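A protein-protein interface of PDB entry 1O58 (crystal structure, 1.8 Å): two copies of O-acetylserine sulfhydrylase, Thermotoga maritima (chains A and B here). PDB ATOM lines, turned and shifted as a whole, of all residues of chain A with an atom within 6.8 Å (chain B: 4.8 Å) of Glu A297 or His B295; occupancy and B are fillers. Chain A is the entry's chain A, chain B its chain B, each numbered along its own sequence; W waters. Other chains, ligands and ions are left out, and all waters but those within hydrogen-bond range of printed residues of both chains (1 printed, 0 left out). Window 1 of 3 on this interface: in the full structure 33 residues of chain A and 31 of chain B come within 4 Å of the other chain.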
ATOM      1  N   GLU A 102     -24.374  -7.410   4.734  1.00  0.00           N
ATOM      2  CA  GLU A 102     -23.047  -6.905   4.395  1.00  0.00           C
ATOM      3  C   GLU A 102     -22.028  -8.045   4.309  1.00  0.00           C
ATOM      4  O   GLU A 102     -21.187  -8.046   3.429  1.00  0.00           O
ATOM      5  CB  GLU A 102     -22.567  -5.886   5.424  1.00  0.00           C
ATOM      6  CG  GLU A 102     -23.282  -4.549   5.367  1.00  0.00           C
ATOM      7  CD  GLU A 102     -24.593  -4.472   6.135  1.00  0.00           C
ATOM      8  OE1 GLU A 102     -25.128  -5.521   6.594  1.00  0.00           O
ATOM      9  OE2 GLU A 102     -25.096  -3.327   6.249  1.00  0.00           O
ATOM     10  N   LEU A 263     -16.237   4.004  14.811  1.00  0.00           N
ATOM     11  CA  LEU A 263     -17.190   3.282  13.993  1.00  0.00           C
ATOM     12  C   LEU A 263     -16.999   1.781  14.201  1.00  0.00           C
ATOM     13  O   LEU A 263     -16.256   1.123  13.463  1.00  0.00           O
ATOM     14  CB  LEU A 263     -16.980   3.622  12.511  1.00  0.00           C
ATOM     15  CG  LEU A 263     -17.310   5.072  12.142  1.00  0.00           C
ATOM     16  CD1 LEU A 263     -16.741   5.434  10.781  1.00  0.00           C
ATOM     17  CD2 LEU A 263     -18.813   5.272  12.176  1.00  0.00           C
ATOM     18  N   VAL A 264     -17.694   1.259  15.203  1.00  0.00           N
ATOM     19  CA  VAL A 264     -17.509  -0.122  15.647  1.00  0.00           C
ATOM     20  C   VAL A 264     -18.826  -0.891  15.525  1.00  0.00           C
ATOM     21  O   VAL A 264     -19.927  -0.297  15.415  1.00  0.00           O
ATOM     22  CB  VAL A 264     -16.959  -0.189  17.091  1.00  0.00           C
ATOM     23  CG1 VAL A 264     -15.614   0.463  17.178  1.00  0.00           C
ATOM     24  CG2 VAL A 264     -17.893   0.396  18.094  1.00  0.00           C
ATOM     25  N   GLY A 265     -18.718  -2.213  15.492  1.00  0.00           N
ATOM     26  CA  GLY A 265     -19.897  -3.065  15.329  1.00  0.00           C
ATOM     27  C   GLY A 265     -20.607  -3.376  16.627  1.00  0.00           C
ATOM     28  O   GLY A 265     -20.265  -2.854  17.690  1.00  0.00           O
ATOM     29  N   ASP A 294     -14.854  -5.440  15.239  1.00  0.00           N
ATOM     30  CA  ASP A 294     -14.999  -5.078  13.815  1.00  0.00           C
ATOM     31  C   ASP A 294     -15.639  -3.707  13.691  1.00  0.00           C
ATOM     32  O   ASP A 294     -15.734  -2.986  14.688  1.00  0.00           O
ATOM     33  CB  ASP A 294     -15.751  -6.169  13.063  1.00  0.00           C
ATOM     34  CG  ASP A 294     -17.210  -6.251  13.446  1.00  0.00           C
ATOM     35  OD1 ASP A 294     -17.698  -5.370  14.205  1.00  0.00           O
ATOM     36  OD2 ASP A 294     -17.950  -7.179  13.036  1.00  0.00           O
ATOM     37  N   HIS A 295     -16.059  -3.340  12.491  1.00  0.00           N
ATOM     38  CA  HIS A 295     -16.483  -1.964  12.211  1.00  0.00           C
ATOM     39  C   HIS A 295     -17.955  -1.791  11.880  1.00  0.00           C
ATOM     40  O   HIS A 295     -18.624  -2.710  11.441  1.00  0.00           O
ATOM     41  CB  HIS A 295     -15.630  -1.352  11.108  1.00  0.00           C
ATOM     42  CG  HIS A 295     -15.843  -1.961   9.762  1.00  0.00           C
ATOM     43  ND1 HIS A 295     -16.631  -1.381   8.797  1.00  0.00           N
ATOM     44  CD2 HIS A 295     -15.300  -3.067   9.195  1.00  0.00           C
ATOM     45  CE1 HIS A 295     -16.619  -2.137   7.712  1.00  0.00           C
ATOM     46  NE2 HIS A 295     -15.840  -3.186   7.939  1.00  0.00           N
ATOM     47  N   ALA A 296     -18.436  -0.567  12.051  1.00  0.00           N
ATOM     48  CA  ALA A 296     -19.880  -0.267  11.972  1.00  0.00           C
ATOM     49  C   ALA A 296     -20.456  -0.440  10.563  1.00  0.00           C
ATOM     50  O   ALA A 296     -21.649  -0.736  10.391  1.00  0.00           O
ATOM     51  CB  ALA A 296     -20.155   1.150  12.458  1.00  0.00           C
ATOM     52  N   GLU A 297     -19.634  -0.240   9.547  1.00  0.00           N
ATOM     53  CA  GLU A 297     -20.148  -0.300   8.175  1.00  0.00           C
ATOM     54  C   GLU A 297     -20.467  -1.727   7.705  1.00  0.00           C
ATOM     55  O   GLU A 297     -21.090  -1.912   6.665  1.00  0.00           O
ATOM     56  CB  GLU A 297     -19.204   0.417   7.200  1.00  0.00           C
ATOM     57  CG  GLU A 297     -19.387   1.933   7.197  1.00  0.00           C
ATOM     58  CD  GLU A 297     -18.293   2.665   6.414  1.00  0.00           C
ATOM     59  OE1 GLU A 297     -18.545   3.136   5.293  1.00  0.00           O
ATOM     60  OE2 GLU A 297     -17.160   2.749   6.935  1.00  0.00           O
ATOM     61  N   ARG A 298     -20.064  -2.727   8.480  1.00  0.00           N
ATOM     62  CA  ARG A 298     -20.499  -4.109   8.264  1.00  0.00           C
ATOM     63  C   ARG A 298     -21.917  -4.376   8.811  1.00  0.00           C
ATOM     64  O   ARG A 298     -22.371  -5.518   8.791  1.00  0.00           O
ATOM     65  CB  ARG A 298     -19.474  -5.036   8.928  1.00  0.00           C
ATOM     66  CG  ARG A 298     -19.541  -6.485   8.521  1.00  0.00           C
ATOM     67  CD  ARG A 298     -18.203  -7.205   8.680  1.00  0.00           C
ATOM     68  NE  ARG A 298     -17.211  -6.711   7.722  1.00  0.00           N
ATOM     69  CZ  ARG A 298     -15.910  -7.055   7.735  1.00  0.00           C
ATOM     70  NH1 ARG A 298     -15.424  -7.877   8.648  1.00  0.00           N
ATOM     71  NH2 ARG A 298     -15.089  -6.580   6.816  1.00  0.00           N
ATOM     72  N   TYR A 299     -22.603  -3.328   9.299  1.00  0.00           N
ATOM     73  CA  TYR A 299     -23.903  -3.467   9.971  1.00  0.00           C
ATOM     74  C   TYR A 299     -24.896  -2.366   9.606  1.00  0.00           C
ATOM     75  O   TYR A 299     -25.920  -2.213  10.274  1.00  0.00           O
ATOM     76  CB  TYR A 299     -23.728  -3.415  11.498  1.00  0.00           C
ATOM     77  CG  TYR A 299     -22.844  -4.498  12.041  1.00  0.00           C
ATOM     78  CD1 TYR A 299     -23.360  -5.728  12.412  1.00  0.00           C
ATOM     79  CD2 TYR A 299     -21.475  -4.296  12.162  1.00  0.00           C
ATOM     80  CE1 TYR A 299     -22.555  -6.705  12.920  1.00  0.00           C
ATOM     81  CE2 TYR A 299     -20.673  -5.276  12.638  1.00  0.00           C
ATOM     82  CZ  TYR A 299     -21.195  -6.479  12.998  1.00  0.00           C
ATOM     83  OH  TYR A 299     -20.373  -7.469  13.466  1.00  0.00           O
ATOM     84  N   LEU A 300     -24.626  -1.601   8.555  1.00  0.00           N
ATOM     85  CA  LEU A 300     -25.488  -0.451   8.254  1.00  0.00           C
ATOM     86  C   LEU A 300     -26.916  -0.871   8.023  1.00  0.00           C
ATOM     87  O   LEU A 300     -27.832  -0.093   8.280  1.00  0.00           O
ATOM     88  CB  LEU A 300     -24.985   0.324   7.049  1.00  0.00           C
ATOM     89  CG  LEU A 300     -23.589   0.913   7.187  1.00  0.00           C
ATOM     90  CD1 LEU A 300     -23.290   1.781   5.962  1.00  0.00           C
ATOM     91  CD2 LEU A 300     -23.414   1.703   8.511  1.00  0.00           C
ATOM     92  N   SER A 301     -27.095  -2.107   7.559  1.00  0.00           N
ATOM     93  CA  SER A 301     -28.404  -2.679   7.307  1.00  0.00           C
ATOM     94  C   SER A 301     -29.273  -2.802   8.560  1.00  0.00           C
ATOM     95  O   SER A 301     -30.504  -2.769   8.467  1.00  0.00           O
ATOM     96  CB  SER A 301     -28.255  -4.053   6.642  1.00  0.00           C
ATOM     97  OG  SER A 301     -27.540  -4.953   7.470  1.00  0.00           O
ATOM     98  N   LEU A 303     -27.967  -1.502  12.114  1.00  0.00           N
ATOM     99  CA  LEU A 303     -27.563  -0.670  13.261  1.00  0.00           C
ATOM    100  C   LEU A 303     -28.073   0.755  13.088  1.00  0.00           C
ATOM    101  O   LEU A 303     -28.514   1.153  12.001  1.00  0.00           O
ATOM    102  CB  LEU A 303     -26.047  -0.668  13.422  1.00  0.00           C
ATOM    103  CG  LEU A 303     -25.467  -0.031  14.688  1.00  0.00           C
ATOM    104  CD1 LEU A 303     -26.129  -0.564  15.980  1.00  0.00           C
ATOM    105  CD2 LEU A 303     -23.977  -0.241  14.708  1.00  0.00           C
ATOM    106  OXT LEU A 303     -28.088   1.538  14.054  1.00  0.00           O
ATOM    107  N   LYS B  39      -7.450   2.986   4.257  1.00  0.00           N
ATOM    108  CA  LYS B  39      -8.643   2.514   5.031  1.00  0.00           C
ATOM    109  C   LYS B  39      -8.337   2.181   6.481  1.00  0.00           C
ATOM    110  O   LYS B  39      -9.266   2.078   7.297  1.00  0.00           O
ATOM    111  CB  LYS B  39      -9.324   1.289   4.384  1.00  0.00           C
ATOM    112  CG  LYS B  39      -8.489   0.005   4.382  1.00  0.00           C
ATOM    113  CD  LYS B  39      -9.165  -1.060   3.485  1.00  0.00           C
ATOM    114  CE  LYS B  39      -8.658  -2.465   3.720  1.00  0.00           C
ATOM    115  NZ  LYS B  39      -9.107  -2.983   5.043  1.00  0.00           N
ATOM    116  N   GLY B  44     -11.751   5.468   8.052  1.00  0.00           N
ATOM    117  CA  GLY B  44     -11.824   4.583   6.900  1.00  0.00           C
ATOM    118  C   GLY B  44     -11.355   5.189   5.599  1.00  0.00           C
ATOM    119  O   GLY B  44     -11.587   4.605   4.519  1.00  0.00           O
ATOM    120  N   GLU B 102     -24.142   4.734   1.769  1.00  0.00           N
ATOM    121  CA  GLU B 102     -23.392   4.312   2.941  1.00  0.00           C
ATOM    122  C   GLU B 102     -22.924   5.553   3.690  1.00  0.00           C
ATOM    123  O   GLU B 102     -22.942   5.592   4.926  1.00  0.00           O
ATOM    124  CB  GLU B 102     -22.189   3.449   2.534  1.00  0.00           C
ATOM    125  CG  GLU B 102     -22.542   2.001   2.184  1.00  0.00           C
ATOM    126  CD  GLU B 102     -22.928   1.769   0.728  1.00  0.00           C
ATOM    127  OE1 GLU B 102     -23.064   2.744  -0.072  1.00  0.00           O
ATOM    128  OE2 GLU B 102     -23.088   0.584   0.379  1.00  0.00           O
ATOM    129  N   VAL B 106     -23.486   6.547   7.710  1.00  0.00           N
ATOM    130  CA  VAL B 106     -22.272   6.780   8.496  1.00  0.00           C
ATOM    131  C   VAL B 106     -22.291   8.189   9.095  1.00  0.00           C
ATOM    132  O   VAL B 106     -21.924   8.373  10.244  1.00  0.00           O
ATOM    133  CB  VAL B 106     -20.976   6.527   7.685  1.00  0.00           C
ATOM    134  CG1 VAL B 106     -19.727   6.992   8.445  1.00  0.00           C
ATOM    135  CG2 VAL B 106     -20.856   5.041   7.313  1.00  0.00           C
ATOM    136  N   LEU B 263      -9.863  -5.050   0.241  1.00  0.00           N
ATOM    137  CA  LEU B 263     -11.240  -4.485   0.194  1.00  0.00           C
ATOM    138  C   LEU B 263     -11.192  -2.963   0.076  1.00  0.00           C
ATOM    139  O   LEU B 263     -11.315  -2.256   1.053  1.00  0.00           O
ATOM    140  CB  LEU B 263     -12.027  -4.908   1.434  1.00  0.00           C
ATOM    141  CG  LEU B 263     -12.353  -6.415   1.502  1.00  0.00           C
ATOM    142  CD1 LEU B 263     -12.801  -6.831   2.917  1.00  0.00           C
ATOM    143  CD2 LEU B 263     -13.405  -6.774   0.471  1.00  0.00           C
ATOM    144  N   VAL B 264     -10.917  -2.504  -1.135  1.00  0.00           N
ATOM    145  CA  VAL B 264     -10.678  -1.093  -1.429  1.00  0.00           C
ATOM    146  C   VAL B 264     -11.822  -0.514  -2.287  1.00  0.00           C
ATOM    147  O   VAL B 264     -12.602  -1.262  -2.915  1.00  0.00           O
ATOM    148  CB  VAL B 264      -9.290  -0.880  -2.076  1.00  0.00           C
ATOM    149  CG1 VAL B 264      -8.194  -1.295  -1.124  1.00  0.00           C
ATOM    150  CG2 VAL B 264      -9.171  -1.616  -3.361  1.00  0.00           C
ATOM    151  N   GLY B 265     -11.962   0.806  -2.256  1.00  0.00           N
ATOM    152  CA  GLY B 265     -13.031   1.494  -2.979  1.00  0.00           C
ATOM    153  C   GLY B 265     -12.720   1.846  -4.423  1.00  0.00           C
ATOM    154  O   GLY B 265     -11.709   1.423  -5.010  1.00  0.00           O
ATOM    155  N   ASP B 294      -9.814   4.580   0.303  1.00  0.00           N
ATOM    156  CA  ASP B 294     -10.825   4.071   1.233  1.00  0.00           C
ATOM    157  C   ASP B 294     -11.161   2.607   0.978  1.00  0.00           C
ATOM    158  O   ASP B 294     -10.439   1.951   0.245  1.00  0.00           O
ATOM    159  CB  ASP B 294     -12.064   4.987   1.237  1.00  0.00           C
ATOM    160  CG  ASP B 294     -12.893   4.944  -0.046  1.00  0.00           C
ATOM    161  OD1 ASP B 294     -12.665   4.118  -0.987  1.00  0.00           O
ATOM    162  OD2 ASP B 294     -13.873   5.725  -0.166  1.00  0.00           O
ATOM    163  N   HIS B 295     -12.250   2.127   1.589  1.00  0.00           N
ATOM    164  CA  HIS B 295     -12.558   0.701   1.659  1.00  0.00           C
ATOM    165  C   HIS B 295     -13.839   0.338   0.917  1.00  0.00           C
ATOM    166  O   HIS B 295     -14.727   1.168   0.635  1.00  0.00           O
ATOM    167  CB  HIS B 295     -12.601   0.217   3.108  1.00  0.00           C
ATOM    168  CG  HIS B 295     -13.760   0.736   3.907  1.00  0.00           C
ATOM    169  ND1 HIS B 295     -14.960   0.060   4.000  1.00  0.00           N
ATOM    170  CD2 HIS B 295     -13.905   1.858   4.658  1.00  0.00           C
ATOM    171  CE1 HIS B 295     -15.797   0.754   4.748  1.00  0.00           C
ATOM    172  NE2 HIS B 295     -15.182   1.844   5.172  1.00  0.00           N
ATOM    173  N   ALA B 296     -13.900  -0.943   0.584  1.00  0.00           N
ATOM    174  CA  ALA B 296     -14.938  -1.471  -0.292  1.00  0.00           C
ATOM    175  C   ALA B 296     -16.312  -1.425   0.370  1.00  0.00           C
ATOM    176  O   ALA B 296     -17.307  -1.331  -0.332  1.00  0.00           O
ATOM    177  CB  ALA B 296     -14.577  -2.896  -0.700  1.00  0.00           C
ATOM    178  N   GLU B 297     -16.375  -1.486   1.710  1.00  0.00           N
ATOM    179  CA  GLU B 297     -17.667  -1.580   2.383  1.00  0.00           C
ATOM    180  C   GLU B 297     -18.415  -0.259   2.359  1.00  0.00           C
ATOM    181  O   GLU B 297     -19.604  -0.224   2.666  1.00  0.00           O
ATOM    182  CB  GLU B 297     -17.564  -2.163   3.795  1.00  0.00           C
ATOM    183  CG  GLU B 297     -17.573  -3.693   3.752  1.00  0.00           C
ATOM    184  CD  GLU B 297     -17.148  -4.327   5.045  1.00  0.00           C
ATOM    185  OE1 GLU B 297     -18.049  -4.859   5.734  1.00  0.00           O
ATOM    186  OE2 GLU B 297     -15.915  -4.324   5.341  1.00  0.00           O
ATOM    187  N   ARG B 298     -17.736   0.798   1.927  1.00  0.00           N
ATOM    188  CA  ARG B 298     -18.397   2.084   1.695  1.00  0.00           C
ATOM    189  C   ARG B 298     -19.165   2.132   0.362  1.00  0.00           C
ATOM    190  O   ARG B 298     -19.808   3.147   0.046  1.00  0.00           O
ATOM    191  CB  ARG B 298     -17.347   3.202   1.803  1.00  0.00           C
ATOM    192  CG  ARG B 298     -17.872   4.552   2.221  1.00  0.00           C
ATOM    193  CD  ARG B 298     -16.791   5.410   2.881  1.00  0.00           C
ATOM    194  NE  ARG B 298     -16.662   5.059   4.298  1.00  0.00           N
ATOM    195  CZ  ARG B 298     -15.789   5.607   5.139  1.00  0.00           C
ATOM    196  NH1 ARG B 298     -14.924   6.502   4.698  1.00  0.00           N
ATOM    197  NH2 ARG B 298     -15.747   5.223   6.418  1.00  0.00           N
ATOM    198  N   TYR B 299     -19.083   1.064  -0.430  1.00  0.00           N
ATOM    199  CA  TYR B 299     -19.652   1.028  -1.759  1.00  0.00           C
ATOM    200  C   TYR B 299     -20.422  -0.267  -2.031  1.00  0.00           C
ATOM    201  O   TYR B 299     -20.567  -0.663  -3.198  1.00  0.00           O
ATOM    202  CB  TYR B 299     -18.548   1.172  -2.817  1.00  0.00           C
ATOM    203  CG  TYR B 299     -17.711   2.425  -2.637  1.00  0.00           C
ATOM    204  CD1 TYR B 299     -18.101   3.629  -3.173  1.00  0.00           C
ATOM    205  CD2 TYR B 299     -16.548   2.387  -1.887  1.00  0.00           C
ATOM    206  CE1 TYR B 299     -17.344   4.785  -2.981  1.00  0.00           C
ATOM    207  CE2 TYR B 299     -15.793   3.493  -1.695  1.00  0.00           C
ATOM    208  CZ  TYR B 299     -16.184   4.699  -2.233  1.00  0.00           C
ATOM    209  OH  TYR B 299     -15.391   5.790  -1.994  1.00  0.00           O
HETATM  210  O   HOH W   1     -21.832  -0.982   4.273  1.00  0.00           O
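Of the 13 printed residues of chain B, 5 touch a printed residue of chain A.
Hydrophobic or aromatic side chains of chain B within 4 Å of the printed part of chain A: Val B106 and His B295.
Hydrophobic or aromatic side chains of chain A within 4 Å of the printed part of chain B: His A295 and Leu A300.
Among the printed residues, Asp or Glu carboxylates within 4 Å of a Lys or Arg side-chain nitrogen of the other chain: Glu A297 with Arg B298 (2.9 Å) and Arg A298 with Glu B297 (2.8 Å).
The side-chain carboxylate (OE2) of Glu A102 lies within hydrogen-bond range of the backbone NH (N) of Leu A300 (2.9 Å).
A ring nitrogen (ND1) of His A295 sits close to the backbone NH of Glu A297, at 3.3 Å.
A ring nitrogen (ND1) of His B295 sits at hydrogen-bond distance from the backbone NH (N) of Glu B297, 3.1 Å away.
His A295 touches Glu B297, and with the chains exchanged Glu A297 touches His B295.
Glu A297 touches Arg B298, and with the chains exchanged Arg A298 touches Glu B297.
Water W1 bridges the backbone carbonyl oxygen (O) of Glu A297 (2.7 Å) and the backbone carbonyl oxygen (O) of Glu B297 (2.8 Å).
A ring nitrogen (NE2) of His A295 lies within hydrogen-bond range of the side-chain carboxylate (OE2) of Glu B297 (2.8 Å).
A ring nitrogen (NE2) of His B295 is in hydrogen-bond range of the side-chain carboxylate (OE2) of Glu A297 (2.8 Å).
The side-chain carboxylate (OE1) of Glu A297 is in salt-bridge range of the guanidinium group (NE) of Arg B298 (2.9 Å).
The guanidinium group of Arg A298 is in salt-bridge range of the side-chain carboxylate of Glu B297 (2.8 Å).
Among the printed residues, merely in contact across the chains: Glu A297 with Val B106 (3.4 Å) and Leu A300 with Glu B102 (3.9 Å).
Glu A297 touches just these residues of chain B: Val B106 (3.4 Å), His B295 (2.8 Å) and Arg B298 (2.9 Å).
His B295 touches just one residue of chain A: Glu A297.
Of the printed residues of chain A, Val B106 touches Glu A297.
Of the printed residues of chain A, Glu B102 touches Leu A300.
Of the printed residues of chain B, Leu A300 touches Glu B102.
Of the printed residues of chain B, Arg A298 touches Glu B297.
Printed residues of chain A within 4 Å of Arg B298: Glu A297.
Tyr B299 touches none of the printed residues of chain A.
The nearest residue of chain B that does not touch Glu A297 is Glu B297 (4.3 Å).
The nearest residue of chain A that does not touch His B295 is His A295 (4.2 Å).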
